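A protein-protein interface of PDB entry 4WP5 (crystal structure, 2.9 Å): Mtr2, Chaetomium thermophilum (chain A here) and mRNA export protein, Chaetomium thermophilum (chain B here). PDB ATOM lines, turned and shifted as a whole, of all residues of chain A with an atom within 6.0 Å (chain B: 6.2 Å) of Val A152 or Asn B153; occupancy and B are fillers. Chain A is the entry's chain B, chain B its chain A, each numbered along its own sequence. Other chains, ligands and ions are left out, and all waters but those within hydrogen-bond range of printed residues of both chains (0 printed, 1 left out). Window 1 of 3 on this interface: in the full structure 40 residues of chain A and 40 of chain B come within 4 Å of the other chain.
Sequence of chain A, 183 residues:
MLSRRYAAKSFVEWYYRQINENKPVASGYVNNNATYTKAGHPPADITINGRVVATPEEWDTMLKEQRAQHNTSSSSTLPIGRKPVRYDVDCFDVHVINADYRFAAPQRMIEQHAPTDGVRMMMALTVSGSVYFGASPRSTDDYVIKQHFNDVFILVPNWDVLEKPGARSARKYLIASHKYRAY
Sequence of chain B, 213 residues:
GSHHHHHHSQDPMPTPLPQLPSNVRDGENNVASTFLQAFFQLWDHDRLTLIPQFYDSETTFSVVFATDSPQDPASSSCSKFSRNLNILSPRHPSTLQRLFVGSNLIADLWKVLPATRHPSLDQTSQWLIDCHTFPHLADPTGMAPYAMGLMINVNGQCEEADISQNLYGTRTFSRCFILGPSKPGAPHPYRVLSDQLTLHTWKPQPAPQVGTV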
ATOM      1  N   LEU A 125      23.622  30.853  12.167  1.00  0.00           N
ATOM      2  CA  LEU A 125      22.696  30.324  11.170  1.00  0.00           C
ATOM      3  C   LEU A 125      23.423  29.510  10.107  1.00  0.00           C
ATOM      4  O   LEU A 125      24.480  29.914   9.621  1.00  0.00           O
ATOM      5  CB  LEU A 125      21.921  31.471  10.512  1.00  0.00           C
ATOM      6  CG  LEU A 125      21.086  31.140   9.271  1.00  0.00           C
ATOM      7  CD1 LEU A 125      20.014  30.113   9.591  1.00  0.00           C
ATOM      8  CD2 LEU A 125      20.469  32.406   8.696  1.00  0.00           C
ATOM      9  N   THR A 126      22.854  28.359   9.762  1.00  0.00           N
ATOM     10  CA  THR A 126      23.337  27.558   8.643  1.00  0.00           C
ATOM     11  C   THR A 126      22.197  27.298   7.665  1.00  0.00           C
ATOM     12  O   THR A 126      21.081  26.977   8.072  1.00  0.00           O
ATOM     13  CB  THR A 126      23.939  26.212   9.108  1.00  0.00           C
ATOM     14  OG1 THR A 126      24.314  25.434   7.965  1.00  0.00           O
ATOM     15  CG2 THR A 126      22.946  25.421   9.954  1.00  0.00           C
ATOM     16  N   VAL A 127      22.486  27.454   6.376  1.00  0.00           N
ATOM     17  CA  VAL A 127      21.500  27.245   5.318  1.00  0.00           C
ATOM     18  C   VAL A 127      22.111  26.383   4.222  1.00  0.00           C
ATOM     19  O   VAL A 127      23.252  26.605   3.817  1.00  0.00           O
ATOM     20  CB  VAL A 127      21.021  28.580   4.710  1.00  0.00           C
ATOM     21  CG1 VAL A 127      19.874  28.341   3.735  1.00  0.00           C
ATOM     22  CG2 VAL A 127      20.602  29.548   5.808  1.00  0.00           C
ATOM     23  N   ASN A 150      26.052  25.733   0.606  1.00  0.00           N
ATOM     24  CA  ASN A 150      25.885  25.688   2.051  1.00  0.00           C
ATOM     25  C   ASN A 150      26.389  26.976   2.683  1.00  0.00           C
ATOM     26  O   ASN A 150      27.594  27.176   2.833  1.00  0.00           O
ATOM     27  CB  ASN A 150      26.623  24.490   2.645  1.00  0.00           C
ATOM     28  CG  ASN A 150      26.712  24.554   4.158  1.00  0.00           C
ATOM     29  OD1 ASN A 150      27.800  24.654   4.724  1.00  0.00           O
ATOM     30  ND2 ASN A 150      25.562  24.515   4.819  1.00  0.00           N
ATOM     31  N   ASP A 151      25.457  27.849   3.047  1.00  0.00           N
ATOM     32  CA  ASP A 151      25.799  29.135   3.637  1.00  0.00           C
ATOM     33  C   ASP A 151      25.839  29.052   5.155  1.00  0.00           C
ATOM     34  O   ASP A 151      25.180  28.206   5.760  1.00  0.00           O
ATOM     35  CB  ASP A 151      24.799  30.207   3.201  1.00  0.00           C
ATOM     36  CG  ASP A 151      25.274  30.996   1.993  1.00  0.00           C
ATOM     37  OD1 ASP A 151      26.439  31.445   1.992  1.00  0.00           O
ATOM     38  OD2 ASP A 151      24.481  31.168   1.043  1.00  0.00           O
ATOM     39  N   VAL A 152      26.619  29.940   5.761  1.00  0.00           N
ATOM     40  CA  VAL A 152      26.710  30.031   7.211  1.00  0.00           C
ATOM     41  C   VAL A 152      26.820  31.495   7.621  1.00  0.00           C
ATOM     42  O   VAL A 152      27.746  32.193   7.205  1.00  0.00           O
ATOM     43  CB  VAL A 152      27.917  29.245   7.757  1.00  0.00           C
ATOM     44  CG1 VAL A 152      28.069  29.472   9.256  1.00  0.00           C
ATOM     45  CG2 VAL A 152      27.770  27.762   7.445  1.00  0.00           C
ATOM     46  N   PHE A 153      25.874  31.950   8.436  1.00  0.00           N
ATOM     47  CA  PHE A 153      25.836  33.342   8.874  1.00  0.00           C
ATOM     48  C   PHE A 153      25.983  33.460  10.385  1.00  0.00           C
ATOM     49  O   PHE A 153      25.670  32.527  11.124  1.00  0.00           O
ATOM     50  CB  PHE A 153      24.524  34.006   8.447  1.00  0.00           C
ATOM     51  CG  PHE A 153      24.294  34.012   6.963  1.00  0.00           C
ATOM     52  CD1 PHE A 153      24.723  35.075   6.186  1.00  0.00           C
ATOM     53  CD2 PHE A 153      23.639  32.960   6.348  1.00  0.00           C
ATOM     54  CE1 PHE A 153      24.505  35.085   4.823  1.00  0.00           C
ATOM     55  CE2 PHE A 153      23.420  32.965   4.986  1.00  0.00           C
ATOM     56  CZ  PHE A 153      23.855  34.027   4.221  1.00  0.00           C
ATOM     57  N   ILE A 154      26.473  34.613  10.831  1.00  0.00           N
ATOM     58  CA  ILE A 154      26.374  35.007  12.231  1.00  0.00           C
ATOM     59  C   ILE A 154      25.540  36.278  12.305  1.00  0.00           C
ATOM     60  O   ILE A 154      25.949  37.328  11.808  1.00  0.00           O
ATOM     61  CB  ILE A 154      27.750  35.241  12.878  1.00  0.00           C
ATOM     62  CG1 ILE A 154      28.533  33.927  12.921  1.00  0.00           C
ATOM     63  CG2 ILE A 154      27.581  35.815  14.285  1.00  0.00           C
ATOM     64  CD1 ILE A 154      29.897  34.032  13.568  1.00  0.00           C
ATOM     65  N   SER A 177      29.119  37.813  10.114  1.00  0.00           N
ATOM     66  CA  SER A 177      30.004  36.829   9.506  1.00  0.00           C
ATOM     67  C   SER A 177      29.258  36.061   8.426  1.00  0.00           C
ATOM     68  O   SER A 177      28.074  35.764   8.577  1.00  0.00           O
ATOM     69  CB  SER A 177      30.548  35.866  10.558  1.00  0.00           C
ATOM     70  OG  SER A 177      31.119  36.571  11.648  1.00  0.00           O
ATOM     71  N   HIS A 178      29.952  35.746   7.338  1.00  0.00           N
ATOM     72  CA  HIS A 178      29.353  35.003   6.236  1.00  0.00           C
ATOM     73  C   HIS A 178      30.355  34.033   5.620  1.00  0.00           C
ATOM     74  O   HIS A 178      31.481  34.410   5.298  1.00  0.00           O
ATOM     75  CB  HIS A 178      28.828  35.963   5.165  1.00  0.00           C
ATOM     76  CG  HIS A 178      28.047  35.288   4.082  1.00  0.00           C
ATOM     77  ND1 HIS A 178      27.714  35.916   2.901  1.00  0.00           N
ATOM     78  CD2 HIS A 178      27.530  34.039   4.001  1.00  0.00           C
ATOM     79  CE1 HIS A 178      27.027  35.084   2.140  1.00  0.00           C
ATOM     80  NE2 HIS A 178      26.901  33.938   2.783  1.00  0.00           N
ATOM     81  N   LYS A 179      29.933  32.780   5.469  1.00  0.00           N
ATOM     82  CA  LYS A 179      30.747  31.749   4.833  1.00  0.00           C
ATOM     83  C   LYS A 179      29.958  31.038   3.741  1.00  0.00           C
ATOM     84  O   LYS A 179      29.089  30.216   4.030  1.00  0.00           O
ATOM     85  CB  LYS A 179      31.232  30.731   5.862  1.00  0.00           C
ATOM     86  CG  LYS A 179      32.627  30.989   6.393  1.00  0.00           C
ATOM     87  CD  LYS A 179      33.102  29.810   7.223  1.00  0.00           C
ATOM     88  CE  LYS A 179      33.214  30.169   8.686  1.00  0.00           C
ATOM     89  NZ  LYS A 179      34.383  31.048   8.925  1.00  0.00           N
ATOM     90  N   TYR A 180      30.266  31.363   2.491  1.00  0.00           N
ATOM     91  CA  TYR A 180      29.596  30.756   1.347  1.00  0.00           C
ATOM     92  C   TYR A 180      30.441  29.626   0.772  1.00  0.00           C
ATOM     93  O   TYR A 180      31.652  29.769   0.598  1.00  0.00           O
ATOM     94  CB  TYR A 180      29.316  31.811   0.272  1.00  0.00           C
ATOM     95  CG  TYR A 180      28.680  31.266  -0.989  1.00  0.00           C
ATOM     96  CD1 TYR A 180      29.460  30.880  -2.071  1.00  0.00           C
ATOM     97  CD2 TYR A 180      27.301  31.148  -1.100  1.00  0.00           C
ATOM     98  CE1 TYR A 180      28.885  30.386  -3.227  1.00  0.00           C
ATOM     99  CE2 TYR A 180      26.717  30.655  -2.251  1.00  0.00           C
ATOM    100  CZ  TYR A 180      27.513  30.276  -3.312  1.00  0.00           C
ATOM    101  OH  TYR A 180      26.938  29.786  -4.461  1.00  0.00           O
ATOM    102  N   ARG A 181      29.794  28.500   0.489  1.00  0.00           N
ATOM    103  CA  ARG A 181      30.444  27.373  -0.170  1.00  0.00           C
ATOM    104  C   ARG A 181      29.511  26.796  -1.219  1.00  0.00           C
ATOM    105  O   ARG A 181      28.312  26.673  -0.985  1.00  0.00           O
ATOM    106  CB  ARG A 181      30.838  26.293   0.843  1.00  0.00           C
ATOM    107  CG  ARG A 181      32.228  26.467   1.436  1.00  0.00           C
ATOM    108  CD  ARG A 181      33.311  26.183   0.405  1.00  0.00           C
ATOM    109  NE  ARG A 181      34.640  26.537   0.891  1.00  0.00           N
ATOM    110  CZ  ARG A 181      35.711  26.674   0.116  1.00  0.00           C
ATOM    111  NH1 ARG A 181      35.624  26.496  -1.196  1.00  0.00           N
ATOM    112  NH2 ARG A 181      36.876  26.999   0.656  1.00  0.00           N
ATOM    113  N   LEU B 128      36.545  20.596   2.829  1.00  0.00           N
ATOM    114  CA  LEU B 128      36.442  22.032   2.599  1.00  0.00           C
ATOM    115  C   LEU B 128      36.221  22.728   3.937  1.00  0.00           C
ATOM    116  O   LEU B 128      35.086  22.893   4.386  1.00  0.00           O
ATOM    117  CB  LEU B 128      35.306  22.354   1.628  1.00  0.00           C
ATOM    118  CG  LEU B 128      35.606  22.091   0.152  1.00  0.00           C
ATOM    119  CD1 LEU B 128      34.318  22.029  -0.651  1.00  0.00           C
ATOM    120  CD2 LEU B 128      36.536  23.160  -0.403  1.00  0.00           C
ATOM    121  N   ILE B 129      37.321  23.128   4.568  1.00  0.00           N
ATOM    122  CA  ILE B 129      37.290  23.667   5.922  1.00  0.00           C
ATOM    123  C   ILE B 129      37.559  25.168   5.945  1.00  0.00           C
ATOM    124  O   ILE B 129      38.699  25.604   5.790  1.00  0.00           O
ATOM    125  CB  ILE B 129      38.329  22.970   6.824  1.00  0.00           C
ATOM    126  CG1 ILE B 129      38.163  21.448   6.764  1.00  0.00           C
ATOM    127  CG2 ILE B 129      38.203  23.467   8.261  1.00  0.00           C
ATOM    128  CD1 ILE B 129      39.342  20.686   7.324  1.00  0.00           C
ATOM    129  N   ASP B 130      36.500  25.945   6.144  1.00  0.00           N
ATOM    130  CA  ASP B 130      36.619  27.388   6.313  1.00  0.00           C
ATOM    131  C   ASP B 130      36.354  27.750   7.768  1.00  0.00           C
ATOM    132  O   ASP B 130      35.424  27.227   8.382  1.00  0.00           O
ATOM    133  CB  ASP B 130      35.646  28.127   5.394  1.00  0.00           C
ATOM    134  CG  ASP B 130      35.887  27.827   3.928  1.00  0.00           C
ATOM    135  OD1 ASP B 130      36.930  27.222   3.605  1.00  0.00           O
ATOM    136  OD2 ASP B 130      35.034  28.206   3.097  1.00  0.00           O
ATOM    137  N   CYS B 131      37.173  28.639   8.317  1.00  0.00           N
ATOM    138  CA  CYS B 131      37.056  29.005   9.724  1.00  0.00           C
ATOM    139  C   CYS B 131      37.662  30.377   9.998  1.00  0.00           C
ATOM    140  O   CYS B 131      38.562  30.823   9.287  1.00  0.00           O
ATOM    141  CB  CYS B 131      37.735  27.951  10.603  1.00  0.00           C
ATOM    142  SG  CYS B 131      39.535  28.094  10.684  1.00  0.00           S
ATOM    143  N   MET B 151      34.603  30.283  14.711  1.00  0.00           N
ATOM    144  CA  MET B 151      33.641  29.578  13.867  1.00  0.00           C
ATOM    145  C   MET B 151      34.382  28.666  12.899  1.00  0.00           C
ATOM    146  O   MET B 151      35.328  29.100  12.246  1.00  0.00           O
ATOM    147  CB  MET B 151      32.767  30.568  13.094  1.00  0.00           C
ATOM    148  CG  MET B 151      31.814  29.912  12.101  1.00  0.00           C
ATOM    149  SD  MET B 151      30.788  31.095  11.209  1.00  0.00           S
ATOM    150  CE  MET B 151      29.214  30.870  12.030  1.00  0.00           C
ATOM    151  N   ILE B 152      33.950  27.410  12.811  1.00  0.00           N
ATOM    152  CA  ILE B 152      34.572  26.436  11.918  1.00  0.00           C
ATOM    153  C   ILE B 152      33.520  25.724  11.073  1.00  0.00           C
ATOM    154  O   ILE B 152      32.811  24.846  11.567  1.00  0.00           O
ATOM    155  CB  ILE B 152      35.379  25.374  12.698  1.00  0.00           C
ATOM    156  CG1 ILE B 152      36.349  26.041  13.679  1.00  0.00           C
ATOM    157  CG2 ILE B 152      36.134  24.467  11.731  1.00  0.00           C
ATOM    158  CD1 ILE B 152      36.970  25.078  14.669  1.00  0.00           C
ATOM    159  N   ASN B 153      33.423  26.102   9.801  1.00  0.00           N
ATOM    160  CA  ASN B 153      32.498  25.450   8.880  1.00  0.00           C
ATOM    161  C   ASN B 153      33.210  24.370   8.072  1.00  0.00           C
ATOM    162  O   ASN B 153      34.184  24.647   7.371  1.00  0.00           O
ATOM    163  CB  ASN B 153      31.860  26.472   7.941  1.00  0.00           C
ATOM    164  CG  ASN B 153      30.718  25.885   7.133  1.00  0.00           C
ATOM    165  OD1 ASN B 153      30.033  24.966   7.582  1.00  0.00           O
ATOM    166  ND2 ASN B 153      30.513  26.409   5.930  1.00  0.00           N
ATOM    167  N   VAL B 154      32.714  23.140   8.178  1.00  0.00           N
ATOM    168  CA  VAL B 154      33.337  21.986   7.535  1.00  0.00           C
ATOM    169  C   VAL B 154      32.397  21.331   6.529  1.00  0.00           C
ATOM    170  O   VAL B 154      31.320  20.862   6.890  1.00  0.00           O
ATOM    171  CB  VAL B 154      33.761  20.925   8.575  1.00  0.00           C
ATOM    172  CG1 VAL B 154      34.386  19.716   7.887  1.00  0.00           C
ATOM    173  CG2 VAL B 154      34.718  21.527   9.596  1.00  0.00           C
ATOM    174  N   ASN B 155      32.815  21.310   5.266  1.00  0.00           N
ATOM    175  CA  ASN B 155      32.105  20.577   4.220  1.00  0.00           C
ATOM    176  C   ASN B 155      32.927  19.373   3.779  1.00  0.00           C
ATOM    177  O   ASN B 155      34.084  19.515   3.388  1.00  0.00           O
ATOM    178  CB  ASN B 155      31.810  21.479   3.020  1.00  0.00           C
ATOM    179  CG  ASN B 155      30.600  22.365   3.235  1.00  0.00           C
ATOM    180  OD1 ASN B 155      29.483  22.009   2.858  1.00  0.00           O
ATOM    181  ND2 ASN B 155      30.817  23.531   3.833  1.00  0.00           N
ATOM    182  N   SER B 174      27.672  18.741   5.744  1.00  0.00           N
ATOM    183  CA  SER B 174      28.277  19.975   6.220  1.00  0.00           C
ATOM    184  C   SER B 174      28.110  20.035   7.732  1.00  0.00           C
ATOM    185  O   SER B 174      27.075  19.627   8.257  1.00  0.00           O
ATOM    186  CB  SER B 174      27.632  21.195   5.563  1.00  0.00           C
ATOM    187  OG  SER B 174      26.697  20.800   4.574  1.00  0.00           O
ATOM    188  N   ARG B 175      29.126  20.533   8.429  1.00  0.00           N
ATOM    189  CA  ARG B 175      29.065  20.644   9.881  1.00  0.00           C
ATOM    190  C   ARG B 175      29.686  21.950  10.359  1.00  0.00           C
ATOM    191  O   ARG B 175      30.840  22.245  10.052  1.00  0.00           O
ATOM    192  CB  ARG B 175      29.765  19.456  10.538  1.00  0.00           C
ATOM    193  CG  ARG B 175      29.432  19.303  12.013  1.00  0.00           C
ATOM    194  CD  ARG B 175      29.730  17.905  12.523  1.00  0.00           C
ATOM    195  NE  ARG B 175      29.163  17.685  13.849  1.00  0.00           N
ATOM    196  CZ  ARG B 175      29.095  16.502  14.449  1.00  0.00           C
ATOM    197  NH1 ARG B 175      29.555  15.417  13.840  1.00  0.00           N
ATOM    198  NH2 ARG B 175      28.559  16.401  15.657  1.00  0.00           N
ATOM    199  N   CYS B 176      28.912  22.722  11.114  1.00  0.00           N
ATOM    200  CA  CYS B 176      29.369  24.009  11.634  1.00  0.00           C
ATOM    201  C   CYS B 176      29.612  23.945  13.138  1.00  0.00           C
ATOM    202  O   CYS B 176      28.715  23.594  13.907  1.00  0.00           O
ATOM    203  CB  CYS B 176      28.348  25.104  11.320  1.00  0.00           C
ATOM    204  SG  CYS B 176      28.955  26.784  11.602  1.00  0.00           S
ATOM    205  N   PHE B 177      30.829  24.290  13.543  1.00  0.00           N
ATOM    206  CA  PHE B 177      31.204  24.334  14.952  1.00  0.00           C
ATOM    207  C   PHE B 177      31.395  25.774  15.411  1.00  0.00           C
ATOM    208  O   PHE B 177      32.117  26.541  14.773  1.00  0.00           O
ATOM    209  CB  PHE B 177      32.499  23.552  15.193  1.00  0.00           C
ATOM    210  CG  PHE B 177      32.394  22.082  14.901  1.00  0.00           C
ATOM    211  CD1 PHE B 177      31.960  21.197  15.875  1.00  0.00           C
ATOM    212  CD2 PHE B 177      32.748  21.581  13.658  1.00  0.00           C
ATOM    213  CE1 PHE B 177      31.871  19.843  15.611  1.00  0.00           C
ATOM    214  CE2 PHE B 177      32.659  20.228  13.389  1.00  0.00           C
ATOM    215  CZ  PHE B 177      32.221  19.359  14.367  1.00  0.00           C
ATOM    216  N   GLN B 196      26.108  22.256  14.473  1.00  0.00           N
ATOM    217  CA  GLN B 196      25.062  22.146  13.460  1.00  0.00           C
ATOM    218  C   GLN B 196      25.455  21.177  12.347  1.00  0.00           C
ATOM    219  O   GLN B 196      26.308  21.494  11.518  1.00  0.00           O
ATOM    220  CB  GLN B 196      24.763  23.521  12.865  1.00  0.00           C
ATOM    221  CG  GLN B 196      24.125  24.492  13.842  1.00  0.00           C
ATOM    222  CD  GLN B 196      24.223  25.932  13.379  1.00  0.00           C
ATOM    223  OE1 GLN B 196      25.307  26.421  13.058  1.00  0.00           O
ATOM    224  NE2 GLN B 196      23.088  26.619  13.335  1.00  0.00           N
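O of Asp B130 lies within hydrogen-bond range of N of Asn B153 (2.7 Å). The backbone NH (N) of Ile A154 lies within hydrogen-bond range of the backbone carbonyl oxygen (O) of Ser A177 (3.0 Å). O of Val A152 lies within hydrogen-bond range of N of Lys A179 (2.9 Å). O of Val A127 sits at hydrogen-bond distance from ND2 of Asn A150, 3.3 Å away. The side-chain amide oxygen of Asn B155 lies close to the side-chain hydroxyl of Ser B174. The backbone carbonyl oxygen (O) of Asn B155 lies within hydrogen-bond range of the backbone NH (N) of Leu B128 (2.7 Å).
Hydrophobic or aromatic side chains of chain B that line the printed part of chain A: Leu B128 and Met B151. Along chain B the printed residues that touch a printed residue of chain A span positions 128 to 196. Among the printed residues, 14 pairs touch across the chains.
The side-chain carboxylate (OD2) of Asp B130 is in salt-bridge range of the guanidinium group (NE) of Arg A181. OD1 of Asn A150 lies within hydrogen-bond range of ND2 of Asn B153 (3.4 Å). The side-chain amide nitrogen (ND2) of Asn B155 is in hydrogen-bond range of the side-chain amide oxygen (OD1) of Asn A150 (3.3 Å).
Among the printed residues, merely in contact across the chains: Ile A154 with Met B151 (3.3 Å), Val A152 with Met B151 (3.3 Å), Val A152 with Asn B153 (3.4 Å), Lys A179 with Cys B131 (3.5 Å), Arg A181 with Leu B128 (3.5 Å), Lys A179 with Asp B130 (3.6 Å), Asn A150 with Ser B174 (3.6 Å), Thr A126 with Gln B196 (3.6 Å), Lys A179 with Met B151 (3.6 Å), Lys A179 with Asn B153 (3.6 Å) and Val A152 with Cys B176 (3.7 Å).
Of chain B, only Met B151, Asn B153 and Cys B176 come within 4 Å of Val A152. Of the printed residues of chain A, Asn B153 touches Asn A150, Val A152 and Lys A179. Of the printed residues of chain B, Asn A150 touches Asn B153, Asn B155 and Ser B174. Of the printed residues of chain B, Arg A181 touches Leu B128 (3.5 Å) and Asp B130 (2.8 Å). Of the printed residues of chain A, Asp B130 touches Lys A179 (3.6 Å) and Arg A181 (2.8 Å). Arg B175 touches none of the printed residues of chain A.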
